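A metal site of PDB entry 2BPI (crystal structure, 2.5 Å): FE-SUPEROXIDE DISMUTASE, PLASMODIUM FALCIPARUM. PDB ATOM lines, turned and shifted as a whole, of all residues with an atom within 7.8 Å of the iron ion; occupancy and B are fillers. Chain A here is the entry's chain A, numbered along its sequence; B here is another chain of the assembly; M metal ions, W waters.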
ATOM      1  N   HIS A  27     -36.353  21.774 -20.284  1.00  0.00           N
ATOM      2  CA  HIS A  27     -35.243  21.997 -19.377  1.00  0.00           C
ATOM      3  C   HIS A  27     -35.749  22.551 -18.034  1.00  0.00           C
ATOM      4  O   HIS A  27     -35.470  21.958 -16.974  1.00  0.00           O
ATOM      5  CB  HIS A  27     -34.184  22.918 -20.012  1.00  0.00           C
ATOM      6  CG  HIS A  27     -32.817  22.799 -19.391  1.00  0.00           C
ATOM      7  ND1 HIS A  27     -31.688  23.301 -19.993  1.00  0.00           N
ATOM      8  CD2 HIS A  27     -32.416  22.247 -18.216  1.00  0.00           C
ATOM      9  CE1 HIS A  27     -30.638  23.067 -19.210  1.00  0.00           C
ATOM     10  NE2 HIS A  27     -31.055  22.431 -18.137  1.00  0.00           N
ATOM     11  N   TYR A  28     -36.529  23.623 -18.096  1.00  0.00           N
ATOM     12  CA  TYR A  28     -37.094  24.279 -16.906  1.00  0.00           C
ATOM     13  C   TYR A  28     -38.323  23.567 -16.278  1.00  0.00           C
ATOM     14  O   TYR A  28     -38.307  23.225 -15.088  1.00  0.00           O
ATOM     15  CB  TYR A  28     -37.399  25.775 -17.198  1.00  0.00           C
ATOM     16  CG  TYR A  28     -37.986  26.544 -16.004  1.00  0.00           C
ATOM     17  CD1 TYR A  28     -37.167  27.024 -14.961  1.00  0.00           C
ATOM     18  CD2 TYR A  28     -39.353  26.785 -15.933  1.00  0.00           C
ATOM     19  CE1 TYR A  28     -37.723  27.726 -13.868  1.00  0.00           C
ATOM     20  CE2 TYR A  28     -39.927  27.488 -14.854  1.00  0.00           C
ATOM     21  CZ  TYR A  28     -39.115  27.949 -13.831  1.00  0.00           C
ATOM     22  OH  TYR A  28     -39.741  28.632 -12.803  1.00  0.00           O
ATOM     23  N   HIS A  31     -37.154  18.985 -16.390  1.00  0.00           N
ATOM     24  CA  HIS A  31     -35.918  18.715 -15.636  1.00  0.00           C
ATOM     25  C   HIS A  31     -35.827  19.463 -14.316  1.00  0.00           C
ATOM     26  O   HIS A  31     -35.760  18.827 -13.283  1.00  0.00           O
ATOM     27  CB  HIS A  31     -34.673  18.914 -16.493  1.00  0.00           C
ATOM     28  CG  HIS A  31     -34.572  17.940 -17.618  1.00  0.00           C
ATOM     29  ND1 HIS A  31     -34.277  16.620 -17.415  1.00  0.00           N
ATOM     30  CD2 HIS A  31     -34.734  18.094 -18.948  1.00  0.00           C
ATOM     31  CE1 HIS A  31     -34.255  15.986 -18.584  1.00  0.00           C
ATOM     32  NE2 HIS A  31     -34.539  16.860 -19.532  1.00  0.00           N
ATOM     33  N   HIS A  32     -35.893  20.798 -14.361  1.00  0.00           N
ATOM     34  CA  HIS A  32     -35.646  21.633 -13.174  1.00  0.00           C
ATOM     35  C   HIS A  32     -36.743  21.442 -12.120  1.00  0.00           C
ATOM     36  O   HIS A  32     -36.435  21.210 -10.935  1.00  0.00           O
ATOM     37  CB  HIS A  32     -35.392  23.103 -13.551  1.00  0.00           C
ATOM     38  CG  HIS A  32     -34.776  23.938 -12.459  1.00  0.00           C
ATOM     39  ND1 HIS A  32     -34.577  25.303 -12.566  1.00  0.00           N
ATOM     40  CD2 HIS A  32     -34.327  23.603 -11.213  1.00  0.00           C
ATOM     41  CE1 HIS A  32     -34.027  25.766 -11.462  1.00  0.00           C
ATOM     42  NE2 HIS A  32     -33.860  24.754 -10.630  1.00  0.00           N
ATOM     43  N   TYR A  35     -36.369  17.929 -10.429  1.00  0.00           N
ATOM     44  CA  TYR A  35     -35.441  18.013  -9.301  1.00  0.00           C
ATOM     45  C   TYR A  35     -36.067  18.581  -8.014  1.00  0.00           C
ATOM     46  O   TYR A  35     -35.731  18.124  -6.911  1.00  0.00           O
ATOM     47  CB  TYR A  35     -34.176  18.807  -9.665  1.00  0.00           C
ATOM     48  CG  TYR A  35     -33.328  18.199 -10.780  1.00  0.00           C
ATOM     49  CD1 TYR A  35     -32.866  16.887 -10.691  1.00  0.00           C
ATOM     50  CD2 TYR A  35     -32.933  18.955 -11.886  1.00  0.00           C
ATOM     51  CE1 TYR A  35     -32.068  16.339 -11.682  1.00  0.00           C
ATOM     52  CE2 TYR A  35     -32.144  18.419 -12.894  1.00  0.00           C
ATOM     53  CZ  TYR A  35     -31.727  17.112 -12.782  1.00  0.00           C
ATOM     54  OH  TYR A  35     -30.947  16.573 -13.763  1.00  0.00           O
ATOM     55  N   GLN A  70     -28.600  20.247  -8.210  1.00  0.00           N
ATOM     56  CA  GLN A  70     -29.139  20.524  -9.547  1.00  0.00           C
ATOM     57  C   GLN A  70     -30.190  21.624  -9.558  1.00  0.00           C
ATOM     58  O   GLN A  70     -30.306  22.341 -10.547  1.00  0.00           O
ATOM     59  CB  GLN A  70     -29.697  19.260 -10.220  1.00  0.00           C
ATOM     60  CG  GLN A  70     -28.649  18.237 -10.713  1.00  0.00           C
ATOM     61  CD  GLN A  70     -27.941  18.653 -11.986  1.00  0.00           C
ATOM     62  OE1 GLN A  70     -26.945  19.363 -11.934  1.00  0.00           O
ATOM     63  NE2 GLN A  70     -28.446  18.214 -13.139  1.00  0.00           N
ATOM     64  N   ASN A  73     -27.953  24.625  -9.197  1.00  0.00           N
ATOM     65  CA  ASN A  73     -27.139  24.818 -10.404  1.00  0.00           C
ATOM     66  C   ASN A  73     -27.992  25.344 -11.568  1.00  0.00           C
ATOM     67  O   ASN A  73     -27.527  26.140 -12.396  1.00  0.00           O
ATOM     68  CB  ASN A  73     -26.408  23.526 -10.813  1.00  0.00           C
ATOM     69  CG  ASN A  73     -25.305  23.084  -9.815  1.00  0.00           C
ATOM     70  OD1 ASN A  73     -24.887  23.832  -8.916  1.00  0.00           O
ATOM     71  ND2 ASN A  73     -24.827  21.861  -9.997  1.00  0.00           N
ATOM     72  N   HIS A  74     -29.250  24.920 -11.614  1.00  0.00           N
ATOM     73  CA  HIS A  74     -30.133  25.398 -12.681  1.00  0.00           C
ATOM     74  C   HIS A  74     -30.602  26.844 -12.480  1.00  0.00           C
ATOM     75  O   HIS A  74     -30.588  27.642 -13.444  1.00  0.00           O
ATOM     76  CB  HIS A  74     -31.298  24.415 -12.935  1.00  0.00           C
ATOM     77  CG  HIS A  74     -30.898  23.201 -13.709  1.00  0.00           C
ATOM     78  ND1 HIS A  74     -30.378  22.074 -13.111  1.00  0.00           N
ATOM     79  CD2 HIS A  74     -30.893  22.957 -15.045  1.00  0.00           C
ATOM     80  CE1 HIS A  74     -30.095  21.174 -14.043  1.00  0.00           C
ATOM     81  NE2 HIS A  74     -30.395  21.681 -15.225  1.00  0.00           N
ATOM     82  N   TYR A  77     -27.953  28.884 -13.547  1.00  0.00           N
ATOM     83  CA  TYR A  77     -27.830  28.780 -15.000  1.00  0.00           C
ATOM     84  C   TYR A  77     -28.778  29.758 -15.674  1.00  0.00           C
ATOM     85  O   TYR A  77     -28.367  30.556 -16.543  1.00  0.00           O
ATOM     86  CB  TYR A  77     -28.054  27.330 -15.470  1.00  0.00           C
ATOM     87  CG  TYR A  77     -28.229  27.082 -16.953  1.00  0.00           C
ATOM     88  CD1 TYR A  77     -27.200  27.319 -17.852  1.00  0.00           C
ATOM     89  CD2 TYR A  77     -29.433  26.539 -17.452  1.00  0.00           C
ATOM     90  CE1 TYR A  77     -27.364  27.071 -19.219  1.00  0.00           C
ATOM     91  CE2 TYR A  77     -29.609  26.264 -18.818  1.00  0.00           C
ATOM     92  CZ  TYR A  77     -28.560  26.539 -19.691  1.00  0.00           C
ATOM     93  OH  TYR A  77     -28.688  26.276 -21.016  1.00  0.00           O
ATOM     94  N   TRP A  78     -30.034  29.718 -15.233  1.00  0.00           N
ATOM     95  CA  TRP A  78     -31.097  30.596 -15.748  1.00  0.00           C
ATOM     96  C   TRP A  78     -30.799  32.070 -15.461  1.00  0.00           C
ATOM     97  O   TRP A  78     -30.916  32.894 -16.378  1.00  0.00           O
ATOM     98  CB  TRP A  78     -32.463  30.201 -15.172  1.00  0.00           C
ATOM     99  CG  TRP A  78     -32.920  28.810 -15.514  1.00  0.00           C
ATOM    100  CD1 TRP A  78     -33.365  27.848 -14.630  1.00  0.00           C
ATOM    101  CD2 TRP A  78     -32.973  28.212 -16.819  1.00  0.00           C
ATOM    102  NE1 TRP A  78     -33.713  26.694 -15.307  1.00  0.00           N
ATOM    103  CE2 TRP A  78     -33.483  26.882 -16.652  1.00  0.00           C
ATOM    104  CE3 TRP A  78     -32.683  28.667 -18.114  1.00  0.00           C
ATOM    105  CZ2 TRP A  78     -33.663  26.008 -17.738  1.00  0.00           C
ATOM    106  CZ3 TRP A  78     -32.868  27.805 -19.200  1.00  0.00           C
ATOM    107  CH2 TRP A  78     -33.348  26.473 -18.993  1.00  0.00           C
ATOM    108  N   GLY A 122     -22.277  17.550 -16.963  1.00  0.00           N
ATOM    109  CA  GLY A 122     -21.626  18.536 -16.107  1.00  0.00           C
ATOM    110  C   GLY A 122     -21.883  19.996 -16.425  1.00  0.00           C
ATOM    111  O   GLY A 122     -22.754  20.335 -17.216  1.00  0.00           O
ATOM    112  N   TRP A 123     -21.093  20.862 -15.803  1.00  0.00           N
ATOM    113  CA  TRP A 123     -21.294  22.277 -15.759  1.00  0.00           C
ATOM    114  C   TRP A 123     -19.952  22.990 -15.977  1.00  0.00           C
ATOM    115  O   TRP A 123     -18.917  22.571 -15.438  1.00  0.00           O
ATOM    116  CB  TRP A 123     -21.798  22.652 -14.359  1.00  0.00           C
ATOM    117  CG  TRP A 123     -23.070  22.058 -14.058  1.00  0.00           C
ATOM    118  CD1 TRP A 123     -23.294  20.799 -13.557  1.00  0.00           C
ATOM    119  CD2 TRP A 123     -24.368  22.635 -14.289  1.00  0.00           C
ATOM    120  NE1 TRP A 123     -24.644  20.580 -13.425  1.00  0.00           N
ATOM    121  CE2 TRP A 123     -25.323  21.680 -13.885  1.00  0.00           C
ATOM    122  CE3 TRP A 123     -24.802  23.873 -14.784  1.00  0.00           C
ATOM    123  CZ2 TRP A 123     -26.710  21.918 -13.965  1.00  0.00           C
ATOM    124  CZ3 TRP A 123     -26.162  24.121 -14.853  1.00  0.00           C
ATOM    125  CH2 TRP A 123     -27.102  23.133 -14.455  1.00  0.00           C
ATOM    126  N   ASP A 158     -24.704  25.091 -18.251  1.00  0.00           N
ATOM    127  CA  ASP A 158     -25.094  23.644 -18.244  1.00  0.00           C
ATOM    128  C   ASP A 158     -24.584  22.935 -19.504  1.00  0.00           C
ATOM    129  O   ASP A 158     -24.764  23.442 -20.644  1.00  0.00           O
ATOM    130  CB  ASP A 158     -26.627  23.522 -18.120  1.00  0.00           C
ATOM    131  CG  ASP A 158     -27.110  22.085 -17.775  1.00  0.00           C
ATOM    132  OD1 ASP A 158     -26.274  21.164 -17.684  1.00  0.00           O
ATOM    133  OD2 ASP A 158     -28.359  21.890 -17.604  1.00  0.00           O
ATOM    134  N   ILE A 159     -23.963  21.760 -19.314  1.00  0.00           N
ATOM    135  CA  ILE A 159     -23.373  20.987 -20.425  1.00  0.00           C
ATOM    136  C   ILE A 159     -23.988  19.570 -20.629  1.00  0.00           C
ATOM    137  O   ILE A 159     -23.685  18.851 -21.587  1.00  0.00           O
ATOM    138  CB  ILE A 159     -21.788  21.065 -20.376  1.00  0.00           C
ATOM    139  CG1 ILE A 159     -21.294  21.596 -21.713  1.00  0.00           C
ATOM    140  CG2 ILE A 159     -21.060  19.756 -19.921  1.00  0.00           C
ATOM    141  CD1 ILE A 159     -21.956  22.901 -22.100  1.00  0.00           C
ATOM    142  N   TRP A 160     -24.901  19.210 -19.732  1.00  0.00           N
ATOM    143  CA  TRP A 160     -25.723  18.018 -19.895  1.00  0.00           C
ATOM    144  C   TRP A 160     -26.348  18.103 -21.260  1.00  0.00           C
ATOM    145  O   TRP A 160     -26.664  19.196 -21.736  1.00  0.00           O
ATOM    146  CB  TRP A 160     -26.832  17.990 -18.827  1.00  0.00           C
ATOM    147  CG  TRP A 160     -26.400  17.668 -17.405  1.00  0.00           C
ATOM    148  CD1 TRP A 160     -25.443  18.313 -16.643  1.00  0.00           C
ATOM    149  CD2 TRP A 160     -26.917  16.617 -16.570  1.00  0.00           C
ATOM    150  NE1 TRP A 160     -25.365  17.740 -15.381  1.00  0.00           N
ATOM    151  CE2 TRP A 160     -26.237  16.686 -15.320  1.00  0.00           C
ATOM    152  CE3 TRP A 160     -27.890  15.625 -16.750  1.00  0.00           C
ATOM    153  CZ2 TRP A 160     -26.501  15.789 -14.266  1.00  0.00           C
ATOM    154  CZ3 TRP A 160     -28.163  14.747 -15.690  1.00  0.00           C
ATOM    155  CH2 TRP A 160     -27.471  14.843 -14.470  1.00  0.00           C
ATOM    156  N   GLU A 161     -26.536  16.957 -21.887  1.00  0.00           N
ATOM    157  CA  GLU A 161     -27.004  16.927 -23.247  1.00  0.00           C
ATOM    158  C   GLU A 161     -28.408  17.513 -23.363  1.00  0.00           C
ATOM    159  O   GLU A 161     -28.743  18.109 -24.375  1.00  0.00           O
ATOM    160  CB  GLU A 161     -26.927  15.519 -23.854  1.00  0.00           C
ATOM    161  CG  GLU A 161     -25.507  15.044 -24.089  1.00  0.00           C
ATOM    162  CD  GLU A 161     -25.377  13.585 -24.518  1.00  0.00           C
ATOM    163  OE1 GLU A 161     -26.069  12.695 -23.976  1.00  0.00           O
ATOM    164  OE2 GLU A 161     -24.543  13.311 -25.406  1.00  0.00           O
ATOM    165  N   HIS A 162     -29.224  17.360 -22.334  1.00  0.00           N
ATOM    166  CA  HIS A 162     -30.582  17.958 -22.350  1.00  0.00           C
ATOM    167  C   HIS A 162     -30.612  19.484 -22.557  1.00  0.00           C
ATOM    168  O   HIS A 162     -31.585  20.032 -23.091  1.00  0.00           O
ATOM    169  CB  HIS A 162     -31.445  17.527 -21.133  1.00  0.00           C
ATOM    170  CG  HIS A 162     -30.972  18.019 -19.805  1.00  0.00           C
ATOM    171  ND1 HIS A 162     -30.636  17.159 -18.769  1.00  0.00           N
ATOM    172  CD2 HIS A 162     -30.835  19.271 -19.297  1.00  0.00           C
ATOM    173  CE1 HIS A 162     -30.301  17.858 -17.700  1.00  0.00           C
ATOM    174  NE2 HIS A 162     -30.435  19.145 -17.986  1.00  0.00           N
ATOM    175  N   ALA A 163     -29.527  20.160 -22.176  1.00  0.00           N
ATOM    176  CA  ALA A 163     -29.475  21.592 -22.267  1.00  0.00           C
ATOM    177  C   ALA A 163     -29.480  22.013 -23.739  1.00  0.00           C
ATOM    178  O   ALA A 163     -29.911  23.135 -24.064  1.00  0.00           O
ATOM    179  CB  ALA A 163     -28.289  22.134 -21.518  1.00  0.00           C
ATOM    180  N   TYR A 164     -29.046  21.119 -24.624  1.00  0.00           N
ATOM    181  CA  TYR A 164     -28.885  21.521 -26.032  1.00  0.00           C
ATOM    182  C   TYR A 164     -29.352  20.509 -27.067  1.00  0.00           C
ATOM    183  O   TYR A 164     -29.450  20.851 -28.226  1.00  0.00           O
ATOM    184  CB  TYR A 164     -27.411  21.881 -26.354  1.00  0.00           C
ATOM    185  CG  TYR A 164     -26.398  20.789 -26.083  1.00  0.00           C
ATOM    186  CD1 TYR A 164     -26.029  19.905 -27.074  1.00  0.00           C
ATOM    187  CD2 TYR A 164     -25.791  20.649 -24.821  1.00  0.00           C
ATOM    188  CE1 TYR A 164     -25.112  18.896 -26.843  1.00  0.00           C
ATOM    189  CE2 TYR A 164     -24.825  19.659 -24.587  1.00  0.00           C
ATOM    190  CZ  TYR A 164     -24.492  18.784 -25.611  1.00  0.00           C
ATOM    191  OH  TYR A 164     -23.570  17.791 -25.438  1.00  0.00           O
ATOM    192  N   TYR A 175     -24.010  25.067 -29.467  1.00  0.00           N
ATOM    193  CA  TYR A 175     -24.727  25.499 -28.279  1.00  0.00           C
ATOM    194  C   TYR A 175     -23.869  26.486 -27.485  1.00  0.00           C
ATOM    195  O   TYR A 175     -24.358  27.508 -27.050  1.00  0.00           O
ATOM    196  CB  TYR A 175     -25.141  24.314 -27.430  1.00  0.00           C
ATOM    197  CG  TYR A 175     -25.476  24.594 -25.988  1.00  0.00           C
ATOM    198  CD1 TYR A 175     -26.672  25.218 -25.627  1.00  0.00           C
ATOM    199  CD2 TYR A 175     -24.596  24.213 -24.949  1.00  0.00           C
ATOM    200  CE1 TYR A 175     -26.987  25.459 -24.257  1.00  0.00           C
ATOM    201  CE2 TYR A 175     -24.915  24.452 -23.596  1.00  0.00           C
ATOM    202  CZ  TYR A 175     -26.110  25.060 -23.252  1.00  0.00           C
ATOM    203  OH  TYR A 175     -26.418  25.265 -21.921  1.00  0.00           O
ATOM    204  N   GLU B 161     -28.213  10.739 -22.389  1.00  0.00           N
ATOM    205  CA  GLU B 161     -29.425  11.382 -22.816  1.00  0.00           C
ATOM    206  C   GLU B 161     -29.514  11.355 -24.328  1.00  0.00           C
ATOM    207  O   GLU B 161     -30.602  11.322 -24.897  1.00  0.00           O
ATOM    208  CB  GLU B 161     -29.551  12.808 -22.247  1.00  0.00           C
ATOM    209  CG  GLU B 161     -29.369  12.855 -20.730  1.00  0.00           C
ATOM    210  CD  GLU B 161     -29.739  14.197 -20.128  1.00  0.00           C
ATOM    211  OE1 GLU B 161     -29.060  15.201 -20.489  1.00  0.00           O
ATOM    212  OE2 GLU B 161     -30.697  14.235 -19.302  1.00  0.00           O
HETATM  213 FE    FE M   1     -29.762  20.883 -17.055  1.00  0.00          FE
HETATM  214  O   HOH W   1     -28.194  19.713 -16.175  1.00  0.00           O
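Water W1 lies within hydrogen-bond range of the side-chain carboxylate (OD1) of Asp 158 (2.8 Å) and the side-chain amide nitrogen (NE2) of Gln 70 (3.4 Å).
The backbone NH (N) of Trp 160 is in hydrogen-bond range of the side-chain carboxylate (OD1) of Asp 158 (3.1 Å). The backbone carbonyl oxygen (O) of Asp 158 sits at hydrogen-bond distance from the side-chain hydroxyl (OH) of Tyr 175. N of His 162 sits at hydrogen-bond distance from OE1 of Glu 161 of chain B (2.8 Å). The backbone carbonyl oxygen (O) of Gln 70 lies within hydrogen-bond range of a ring nitrogen (ND1) of His 74 (2.6 Å). The backbone carbonyl oxygen of His 27 sits at hydrogen-bond distance from the backbone NH of His 32 (2.9 Å).
Four residues have an atom within 4 Å of the iron ion: His 27, His 74, Asp 158 and His 162.
The side-chain carboxylate (OD2) of Asp 158 binds the iron ion, 1.8 Å away. NE2 of His 162 is bound to the iron ion, at 2.1 Å. NE2 of His 74 is bound to the iron ion, at 2.1 Å. The iron ion is bound by water W1 (2.1 Å). NE2 of His 27 is bound to the iron ion (2.3 Å). The iron ion has five donor atoms within binding distance.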
